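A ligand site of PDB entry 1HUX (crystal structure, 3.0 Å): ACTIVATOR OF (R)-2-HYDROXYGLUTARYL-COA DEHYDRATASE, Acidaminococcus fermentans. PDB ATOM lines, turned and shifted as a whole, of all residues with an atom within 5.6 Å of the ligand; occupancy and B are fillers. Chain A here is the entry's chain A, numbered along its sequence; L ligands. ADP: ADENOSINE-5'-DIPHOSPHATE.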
ATOM      1  N   ASP A   9       8.475 -16.069  36.290  1.00  0.00           N
ATOM      2  CA  ASP A   9       8.076 -17.406  35.854  1.00  0.00           C
ATOM      3  C   ASP A   9       9.306 -18.185  35.407  1.00  0.00           C
ATOM      4  O   ASP A   9       9.747 -18.035  34.273  1.00  0.00           O
ATOM      5  CB  ASP A   9       7.098 -17.279  34.681  1.00  0.00           C
ATOM      6  CG  ASP A   9       6.519 -18.612  34.250  1.00  0.00           C
ATOM      7  OD1 ASP A   9       5.858 -18.663  33.191  1.00  0.00           O
ATOM      8  OD2 ASP A   9       6.726 -19.621  34.982  1.00  0.00           O
ATOM      9  N   VAL A  10       9.868 -18.995  36.272  1.00  0.00           N
ATOM     10  CA  VAL A  10      11.052 -19.751  35.887  1.00  0.00           C
ATOM     11  C   VAL A  10      10.704 -21.140  35.355  1.00  0.00           C
ATOM     12  O   VAL A  10      10.472 -22.070  36.124  1.00  0.00           O
ATOM     13  CB  VAL A  10      12.104 -19.840  37.079  1.00  0.00           C
ATOM     14  CG1 VAL A  10      11.386 -19.710  38.419  1.00  0.00           C
ATOM     15  CG2 VAL A  10      12.872 -21.167  37.043  1.00  0.00           C
ATOM     16  N   GLY A  11      10.637 -21.267  34.036  1.00  0.00           N
ATOM     17  CA  GLY A  11      10.304 -22.554  33.434  1.00  0.00           C
ATOM     18  C   GLY A  11      11.501 -23.464  33.231  1.00  0.00           C
ATOM     19  O   GLY A  11      12.604 -23.155  33.670  1.00  0.00           O
ATOM     20  N   SER A  12      11.272 -24.597  32.570  1.00  0.00           N
ATOM     21  CA  SER A  12      12.350 -25.558  32.310  1.00  0.00           C
ATOM     22  C   SER A  12      13.186 -25.139  31.087  1.00  0.00           C
ATOM     23  O   SER A  12      14.356 -25.513  30.946  1.00  0.00           O
ATOM     24  CB  SER A  12      11.744 -26.950  32.076  1.00  0.00           C
ATOM     25  OG  SER A  12      10.857 -26.916  30.975  1.00  0.00           O
ATOM     26  N   THR A  13      12.572 -24.358  30.215  1.00  0.00           N
ATOM     27  CA  THR A  13      13.206 -23.876  28.991  1.00  0.00           C
ATOM     28  C   THR A  13      13.718 -22.449  29.141  1.00  0.00           C
ATOM     29  O   THR A  13      14.820 -22.118  28.733  1.00  0.00           O
ATOM     30  CB  THR A  13      12.187 -23.912  27.807  1.00  0.00           C
ATOM     31  OG1 THR A  13      12.045 -25.262  27.372  1.00  0.00           O
ATOM     32  CG2 THR A  13      12.623 -23.026  26.647  1.00  0.00           C
ATOM     33  N   ALA A  14      12.894 -21.594  29.726  1.00  0.00           N
ATOM     34  CA  ALA A  14      13.286 -20.213  29.870  1.00  0.00           C
ATOM     35  C   ALA A  14      12.745 -19.633  31.153  1.00  0.00           C
ATOM     36  O   ALA A  14      11.926 -20.246  31.825  1.00  0.00           O
ATOM     37  CB  ALA A  14      12.761 -19.421  28.696  1.00  0.00           C
ATOM     38  N   SER A  15      13.212 -18.442  31.473  1.00  0.00           N
ATOM     39  CA  SER A  15      12.779 -17.738  32.662  1.00  0.00           C
ATOM     40  C   SER A  15      12.236 -16.401  32.160  1.00  0.00           C
ATOM     41  O   SER A  15      12.965 -15.638  31.507  1.00  0.00           O
ATOM     42  CB  SER A  15      13.967 -17.524  33.594  1.00  0.00           C
ATOM     43  OG  SER A  15      13.535 -17.149  34.886  1.00  0.00           O
ATOM     44  N   LYS A  16      10.960 -16.150  32.424  1.00  0.00           N
ATOM     45  CA  LYS A  16      10.316 -14.908  31.994  1.00  0.00           C
ATOM     46  C   LYS A  16      10.058 -14.027  33.200  1.00  0.00           C
ATOM     47  O   LYS A  16       9.859 -14.531  34.329  1.00  0.00           O
ATOM     48  CB  LYS A  16       8.981 -15.189  31.273  1.00  0.00           C
ATOM     49  CG  LYS A  16       9.065 -15.779  29.847  1.00  0.00           C
ATOM     50  CD  LYS A  16       9.548 -17.225  29.846  1.00  0.00           C
ATOM     51  CE  LYS A  16       8.678 -18.140  30.691  1.00  0.00           C
ATOM     52  NZ  LYS A  16       9.259 -19.507  30.784  1.00  0.00           N
ATOM     53  N   LEU A  31      13.132 -12.214  29.111  1.00  0.00           N
ATOM     54  CA  LEU A  31      13.150 -13.641  28.854  1.00  0.00           C
ATOM     55  C   LEU A  31      14.585 -14.118  28.674  1.00  0.00           C
ATOM     56  O   LEU A  31      15.309 -13.582  27.829  1.00  0.00           O
ATOM     57  CB  LEU A  31      12.316 -13.935  27.602  1.00  0.00           C
ATOM     58  CG  LEU A  31      12.261 -15.339  27.018  1.00  0.00           C
ATOM     59  CD1 LEU A  31      12.153 -16.420  28.071  1.00  0.00           C
ATOM     60  CD2 LEU A  31      11.070 -15.385  26.116  1.00  0.00           C
ATOM     61  N   GLU A  82       1.938 -22.646  39.043  1.00  0.00           N
ATOM     62  CA  GLU A  82       1.939 -22.176  37.674  1.00  0.00           C
ATOM     63  C   GLU A  82       0.535 -22.142  37.113  1.00  0.00           C
ATOM     64  O   GLU A  82       0.223 -21.304  36.262  1.00  0.00           O
ATOM     65  CB  GLU A  82       2.827 -23.062  36.806  1.00  0.00           C
ATOM     66  CG  GLU A  82       2.989 -22.577  35.369  1.00  0.00           C
ATOM     67  CD  GLU A  82       4.417 -22.261  35.012  1.00  0.00           C
ATOM     68  OE1 GLU A  82       5.299 -23.113  35.260  1.00  0.00           O
ATOM     69  OE2 GLU A  82       4.662 -21.151  34.476  1.00  0.00           O
ATOM     70  N   ASP A 102      -2.090 -24.047  27.742  1.00  0.00           N
ATOM     71  CA  ASP A 102      -0.683 -23.633  27.889  1.00  0.00           C
ATOM     72  C   ASP A 102       0.310 -24.700  27.478  1.00  0.00           C
ATOM     73  O   ASP A 102       0.514 -25.697  28.189  1.00  0.00           O
ATOM     74  CB  ASP A 102      -0.394 -23.240  29.345  1.00  0.00           C
ATOM     75  CG  ASP A 102       1.103 -23.008  29.610  1.00  0.00           C
ATOM     76  OD1 ASP A 102       1.675 -23.707  30.477  1.00  0.00           O
ATOM     77  OD2 ASP A 102       1.687 -22.126  28.939  1.00  0.00           O
ATOM     78  N   ILE A 103       0.959 -24.477  26.333  1.00  0.00           N
ATOM     79  CA  ILE A 103       1.943 -25.439  25.848  1.00  0.00           C
ATOM     80  C   ILE A 103       3.328 -24.846  26.019  1.00  0.00           C
ATOM     81  O   ILE A 103       3.645 -23.780  25.478  1.00  0.00           O
ATOM     82  CB  ILE A 103       1.764 -25.777  24.321  1.00  0.00           C
ATOM     83  CG1 ILE A 103       0.344 -26.290  24.044  1.00  0.00           C
ATOM     84  CG2 ILE A 103       2.764 -26.859  23.910  1.00  0.00           C
ATOM     85  CD1 ILE A 103       0.063 -26.573  22.575  1.00  0.00           C
ATOM     86  N   GLY A 104       4.162 -25.536  26.787  1.00  0.00           N
ATOM     87  CA  GLY A 104       5.520 -25.088  26.987  1.00  0.00           C
ATOM     88  C   GLY A 104       6.426 -26.256  26.675  1.00  0.00           C
ATOM     89  O   GLY A 104       5.941 -27.323  26.317  1.00  0.00           O
ATOM     90  N   GLY A 105       7.741 -26.071  26.783  1.00  0.00           N
ATOM     91  CA  GLY A 105       8.621 -27.195  26.521  1.00  0.00           C
ATOM     92  C   GLY A 105       8.398 -28.164  27.662  1.00  0.00           C
ATOM     93  O   GLY A 105       8.042 -27.747  28.774  1.00  0.00           O
ATOM     94  N   ASP A 107       6.000 -29.980  28.739  1.00  0.00           N
ATOM     95  CA  ASP A 107       4.685 -30.160  29.371  1.00  0.00           C
ATOM     96  C   ASP A 107       3.536 -29.352  28.733  1.00  0.00           C
ATOM     97  O   ASP A 107       3.745 -28.301  28.097  1.00  0.00           O
ATOM     98  CB  ASP A 107       4.775 -29.785  30.857  1.00  0.00           C
ATOM     99  CG  ASP A 107       4.801 -28.295  31.071  1.00  0.00           C
ATOM    100  OD1 ASP A 107       5.712 -27.630  30.530  1.00  0.00           O
ATOM    101  OD2 ASP A 107       3.891 -27.776  31.770  1.00  0.00           O
ATOM    102  N   GLY A 132       6.457 -28.733  23.472  1.00  0.00           N
ATOM    103  CA  GLY A 132       7.291 -28.028  22.524  1.00  0.00           C
ATOM    104  C   GLY A 132       8.505 -28.866  22.202  1.00  0.00           C
ATOM    105  O   GLY A 132       9.224 -28.634  21.220  1.00  0.00           O
ATOM    106  N   ARG A 133       8.736 -29.878  23.046  1.00  0.00           N
ATOM    107  CA  ARG A 133       9.860 -30.776  22.878  1.00  0.00           C
ATOM    108  C   ARG A 133       9.581 -31.698  21.689  1.00  0.00           C
ATOM    109  O   ARG A 133      10.480 -32.153  20.989  1.00  0.00           O
ATOM    110  CB  ARG A 133      10.043 -31.588  24.154  1.00  0.00           C
ATOM    111  CG  ARG A 133      11.180 -32.564  24.102  1.00  0.00           C
ATOM    112  CD  ARG A 133      12.478 -31.882  23.703  1.00  0.00           C
ATOM    113  NE  ARG A 133      13.593 -32.770  23.935  1.00  0.00           N
ATOM    114  CZ  ARG A 133      13.961 -33.197  25.141  1.00  0.00           C
ATOM    115  NH1 ARG A 133      13.295 -32.796  26.231  1.00  0.00           N
ATOM    116  NH2 ARG A 133      14.970 -34.055  25.269  1.00  0.00           N
ATOM    117  N   ASP A 136      10.511 -29.787  18.767  1.00  0.00           N
ATOM    118  CA  ASP A 136      11.951 -29.657  18.607  1.00  0.00           C
ATOM    119  C   ASP A 136      12.480 -30.854  17.859  1.00  0.00           C
ATOM    120  O   ASP A 136      13.086 -30.714  16.793  1.00  0.00           O
ATOM    121  CB  ASP A 136      12.642 -29.560  19.966  1.00  0.00           C
ATOM    122  CG  ASP A 136      12.565 -28.169  20.559  1.00  0.00           C
ATOM    123  OD1 ASP A 136      12.991 -27.205  19.881  1.00  0.00           O
ATOM    124  OD2 ASP A 136      12.071 -28.052  21.704  1.00  0.00           O
ATOM    125  N   VAL A 146      12.576 -24.231  14.767  1.00  0.00           N
ATOM    126  CA  VAL A 146      11.316 -24.319  15.483  1.00  0.00           C
ATOM    127  C   VAL A 146      10.449 -23.071  15.304  1.00  0.00           C
ATOM    128  O   VAL A 146       9.223 -23.168  15.319  1.00  0.00           O
ATOM    129  CB  VAL A 146      11.556 -24.534  16.980  1.00  0.00           C
ATOM    130  CG1 VAL A 146      10.241 -24.540  17.734  1.00  0.00           C
ATOM    131  CG2 VAL A 146      12.284 -25.837  17.183  1.00  0.00           C
ATOM    132  N   SER A 147      11.065 -21.915  15.111  1.00  0.00           N
ATOM    133  CA  SER A 147      10.314 -20.679  14.928  1.00  0.00           C
ATOM    134  C   SER A 147       9.953 -20.423  13.456  1.00  0.00           C
ATOM    135  O   SER A 147       9.433 -19.354  13.097  1.00  0.00           O
ATOM    136  CB  SER A 147      11.100 -19.502  15.491  1.00  0.00           C
ATOM    137  OG  SER A 147      12.487 -19.705  15.306  1.00  0.00           O
ATOM    138  N   ASP A 148      10.223 -21.404  12.615  1.00  0.00           N
ATOM    139  CA  ASP A 148       9.918 -21.294  11.192  1.00  0.00           C
ATOM    140  C   ASP A 148       8.762 -22.220  10.823  1.00  0.00           C
ATOM    141  O   ASP A 148       8.020 -21.967   9.855  1.00  0.00           O
ATOM    142  CB  ASP A 148      11.153 -21.657  10.374  1.00  0.00           C
ATOM    143  CG  ASP A 148      12.164 -20.525  10.311  1.00  0.00           C
ATOM    144  OD1 ASP A 148      13.371 -20.826  10.184  1.00  0.00           O
ATOM    145  OD2 ASP A 148      11.750 -19.339  10.349  1.00  0.00           O
ATOM    146  N   GLY A 216       1.903 -19.789  26.477  1.00  0.00           N
ATOM    147  CA  GLY A 216       3.155 -20.519  26.418  1.00  0.00           C
ATOM    148  C   GLY A 216       3.952 -20.111  25.200  1.00  0.00           C
ATOM    149  O   GLY A 216       3.478 -19.364  24.350  1.00  0.00           O
ATOM    150  N   GLY A 217       5.188 -20.589  25.105  1.00  0.00           N
ATOM    151  CA  GLY A 217       6.002 -20.206  23.979  1.00  0.00           C
ATOM    152  C   GLY A 217       5.451 -20.754  22.685  1.00  0.00           C
ATOM    153  O   GLY A 217       5.387 -20.033  21.684  1.00  0.00           O
ATOM    154  N   VAL A 218       5.050 -22.021  22.702  1.00  0.00           N
ATOM    155  CA  VAL A 218       4.508 -22.636  21.501  1.00  0.00           C
ATOM    156  C   VAL A 218       3.300 -21.848  20.991  1.00  0.00           C
ATOM    157  O   VAL A 218       2.897 -21.980  19.837  1.00  0.00           O
ATOM    158  CB  VAL A 218       4.103 -24.096  21.774  1.00  0.00           C
ATOM    159  CG1 VAL A 218       3.654 -24.751  20.487  1.00  0.00           C
ATOM    160  CG2 VAL A 218       5.285 -24.846  22.378  1.00  0.00           C
ATOM    161  N   ALA A 219       2.730 -21.024  21.863  1.00  0.00           N
ATOM    162  CA  ALA A 219       1.566 -20.225  21.498  1.00  0.00           C
ATOM    163  C   ALA A 219       1.833 -19.462  20.204  1.00  0.00           C
ATOM    164  O   ALA A 219       0.944 -19.307  19.369  1.00  0.00           O
ATOM    165  CB  ALA A 219       1.219 -19.275  22.619  1.00  0.00           C
ATOM    166  N   GLN A 220       3.057 -18.993  20.048  1.00  0.00           N
ATOM    167  CA  GLN A 220       3.442 -18.230  18.862  1.00  0.00           C
ATOM    168  C   GLN A 220       3.174 -18.982  17.580  1.00  0.00           C
ATOM    169  O   GLN A 220       2.691 -18.407  16.587  1.00  0.00           O
ATOM    170  CB  GLN A 220       4.922 -17.865  18.953  1.00  0.00           C
ATOM    171  CG  GLN A 220       5.242 -16.938  20.088  1.00  0.00           C
ATOM    172  CD  GLN A 220       6.691 -16.962  20.438  1.00  0.00           C
ATOM    173  OE1 GLN A 220       7.550 -16.777  19.577  1.00  0.00           O
ATOM    174  NE2 GLN A 220       6.994 -17.191  21.709  1.00  0.00           N
ATOM    175  N   ASN A 221       3.481 -20.285  17.593  1.00  0.00           N
ATOM    176  CA  ASN A 221       3.294 -21.154  16.441  1.00  0.00           C
ATOM    177  C   ASN A 221       1.831 -21.154  16.001  1.00  0.00           C
ATOM    178  O   ASN A 221       1.033 -21.964  16.472  1.00  0.00           O
ATOM    179  CB  ASN A 221       3.723 -22.578  16.801  1.00  0.00           C
ATOM    180  CG  ASN A 221       3.858 -23.482  15.574  1.00  0.00           C
ATOM    181  OD1 ASN A 221       3.050 -23.409  14.640  1.00  0.00           O
ATOM    182  ND2 ASN A 221       4.854 -24.356  15.583  1.00  0.00           N
ATOM    183  N   GLN A 243       3.828 -15.881  25.974  1.00  0.00           N
ATOM    184  CA  GLN A 243       4.856 -16.580  26.750  1.00  0.00           C
ATOM    185  C   GLN A 243       5.185 -15.941  28.093  1.00  0.00           C
ATOM    186  O   GLN A 243       5.875 -16.550  28.930  1.00  0.00           O
ATOM    187  CB  GLN A 243       6.123 -16.721  25.892  1.00  0.00           C
ATOM    188  CG  GLN A 243       7.248 -17.502  26.553  1.00  0.00           C
ATOM    189  CD  GLN A 243       8.412 -17.743  25.596  1.00  0.00           C
ATOM    190  OE1 GLN A 243       8.593 -17.002  24.611  1.00  0.00           O
ATOM    191  NE2 GLN A 243       9.212 -18.763  25.888  1.00  0.00           N
HETATM  192  PB  ADP L   1       8.762 -23.424  30.130  1.00  0.00           P
HETATM  193  O1B ADP L   1       7.369 -23.956  30.292  1.00  0.00           O
HETATM  194  O2B ADP L   1       9.044 -22.093  30.871  1.00  0.00           O
HETATM  195  O3B ADP L   1       9.847 -24.470  30.356  1.00  0.00           O
HETATM  196  PA  ADP L   1       8.158 -21.953  27.794  1.00  0.00           P
HETATM  197  O1A ADP L   1       8.890 -20.643  27.854  1.00  0.00           O
HETATM  198  O2A ADP L   1       6.711 -21.942  28.035  1.00  0.00           O
HETATM  199  O3A ADP L   1       8.915 -23.013  28.725  1.00  0.00           O
HETATM  200  O5' ADP L   1       8.516 -22.663  26.450  1.00  0.00           O
HETATM  201  C5' ADP L   1       8.089 -22.124  25.317  1.00  0.00           C
HETATM  202  C4' ADP L   1       8.170 -23.059  24.160  1.00  0.00           C
HETATM  203  O4' ADP L   1       7.865 -22.321  22.943  1.00  0.00           O
HETATM  204  C3' ADP L   1       9.556 -23.847  23.854  1.00  0.00           C
HETATM  205  O3' ADP L   1       9.296 -25.172  23.310  1.00  0.00           O
HETATM  206  C2' ADP L   1      10.176 -22.851  22.898  1.00  0.00           C
HETATM  207  O2' ADP L   1      11.172 -23.343  21.939  1.00  0.00           O
HETATM  208  C1' ADP L   1       8.943 -22.355  22.137  1.00  0.00           C
HETATM  209  N9  ADP L   1       9.118 -21.153  21.293  1.00  0.00           N
HETATM  210  C8  ADP L   1       9.725 -20.027  21.679  1.00  0.00           C
HETATM  211  N7  ADP L   1       9.736 -19.142  20.778  1.00  0.00           N
HETATM  212  C5  ADP L   1       9.084 -19.737  19.702  1.00  0.00           C
HETATM  213  C6  ADP L   1       8.731 -19.296  18.380  1.00  0.00           C
HETATM  214  N6  ADP L   1       9.042 -18.057  17.904  1.00  0.00           N
HETATM  215  N1  ADP L   1       8.053 -20.164  17.573  1.00  0.00           N
HETATM  216  C2  ADP L   1       7.750 -21.387  18.033  1.00  0.00           C
HETATM  217  N3  ADP L   1       8.033 -21.889  19.259  1.00  0.00           N
HETATM  218  C4  ADP L   1       8.706 -20.997  20.037  1.00  0.00           C
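NE2 of Gln 220 lies within hydrogen-bond range of OE1 of Gln 243 (3.3 Å). NE2 of Gln 220 lies within hydrogen-bond range of O of Gly 217, at 3.3 Å. O of Ala 14 is in hydrogen-bond range of NZ of Lys 16 (3.0 Å). The backbone carbonyl oxygen (O) of Lys 16 is in hydrogen-bond range of the backbone NH (N) of Asp 9, 2.9 Å away. The backbone carbonyl oxygen of Gly 104 lies within hydrogen-bond range of the backbone NH of Gly 132 (3.2 Å).
The side-chain amide oxygen of Gln 220 sits at hydrogen-bond distance from a nitrogen (N6) of the ligand, 2.6 Å away. An oxygen (O2B) of the ligand lies within salt-bridge range of the side-chain amino group (NZ) of Lys 16, 2.6 Å away. The backbone NH (N) of Ser 12 sits at hydrogen-bond distance from an oxygen (O3B) of the ligand, at 2.6 Å. The side-chain hydroxyl (OG) of Ser 12 sits at hydrogen-bond distance from an oxygen (O3B) of the ligand. An oxygen (O3B) of the ligand lies within hydrogen-bond range of the backbone NH (N) of Thr 13 (2.7 Å). NE2 of Gln 243 sits at hydrogen-bond distance from O1A of the ligand (2.7 Å). N of Val 218 sits at hydrogen-bond distance from O4' of the ligand.
CA of Gly 11 touches O2B of the ligand, 2.9 Å away. Ala 14 touches the ligand (O to O2B, 3.6 Å). Gly 104 touches the ligand. Gly 105 touches the ligand (N to O5', 3.5 Å). Gly 132 touches the ligand (CA to O3', 3.6 Å). Val 146 touches the ligand. Ser 147 touches the ligand. Gly 217 touches the ligand. 14 residues have an atom within 4 Å of the ligand: Gly 11, Ser 12, Thr 13, Ala 14, Lys 16, Gly 104, Gly 105, Gly 132, Val 146, Ser 147, Gly 217, Val 218, Gln 220 and Gln 243. The nearest printed residue that does not touch the ligand is Asp 107 (4.04 Å).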
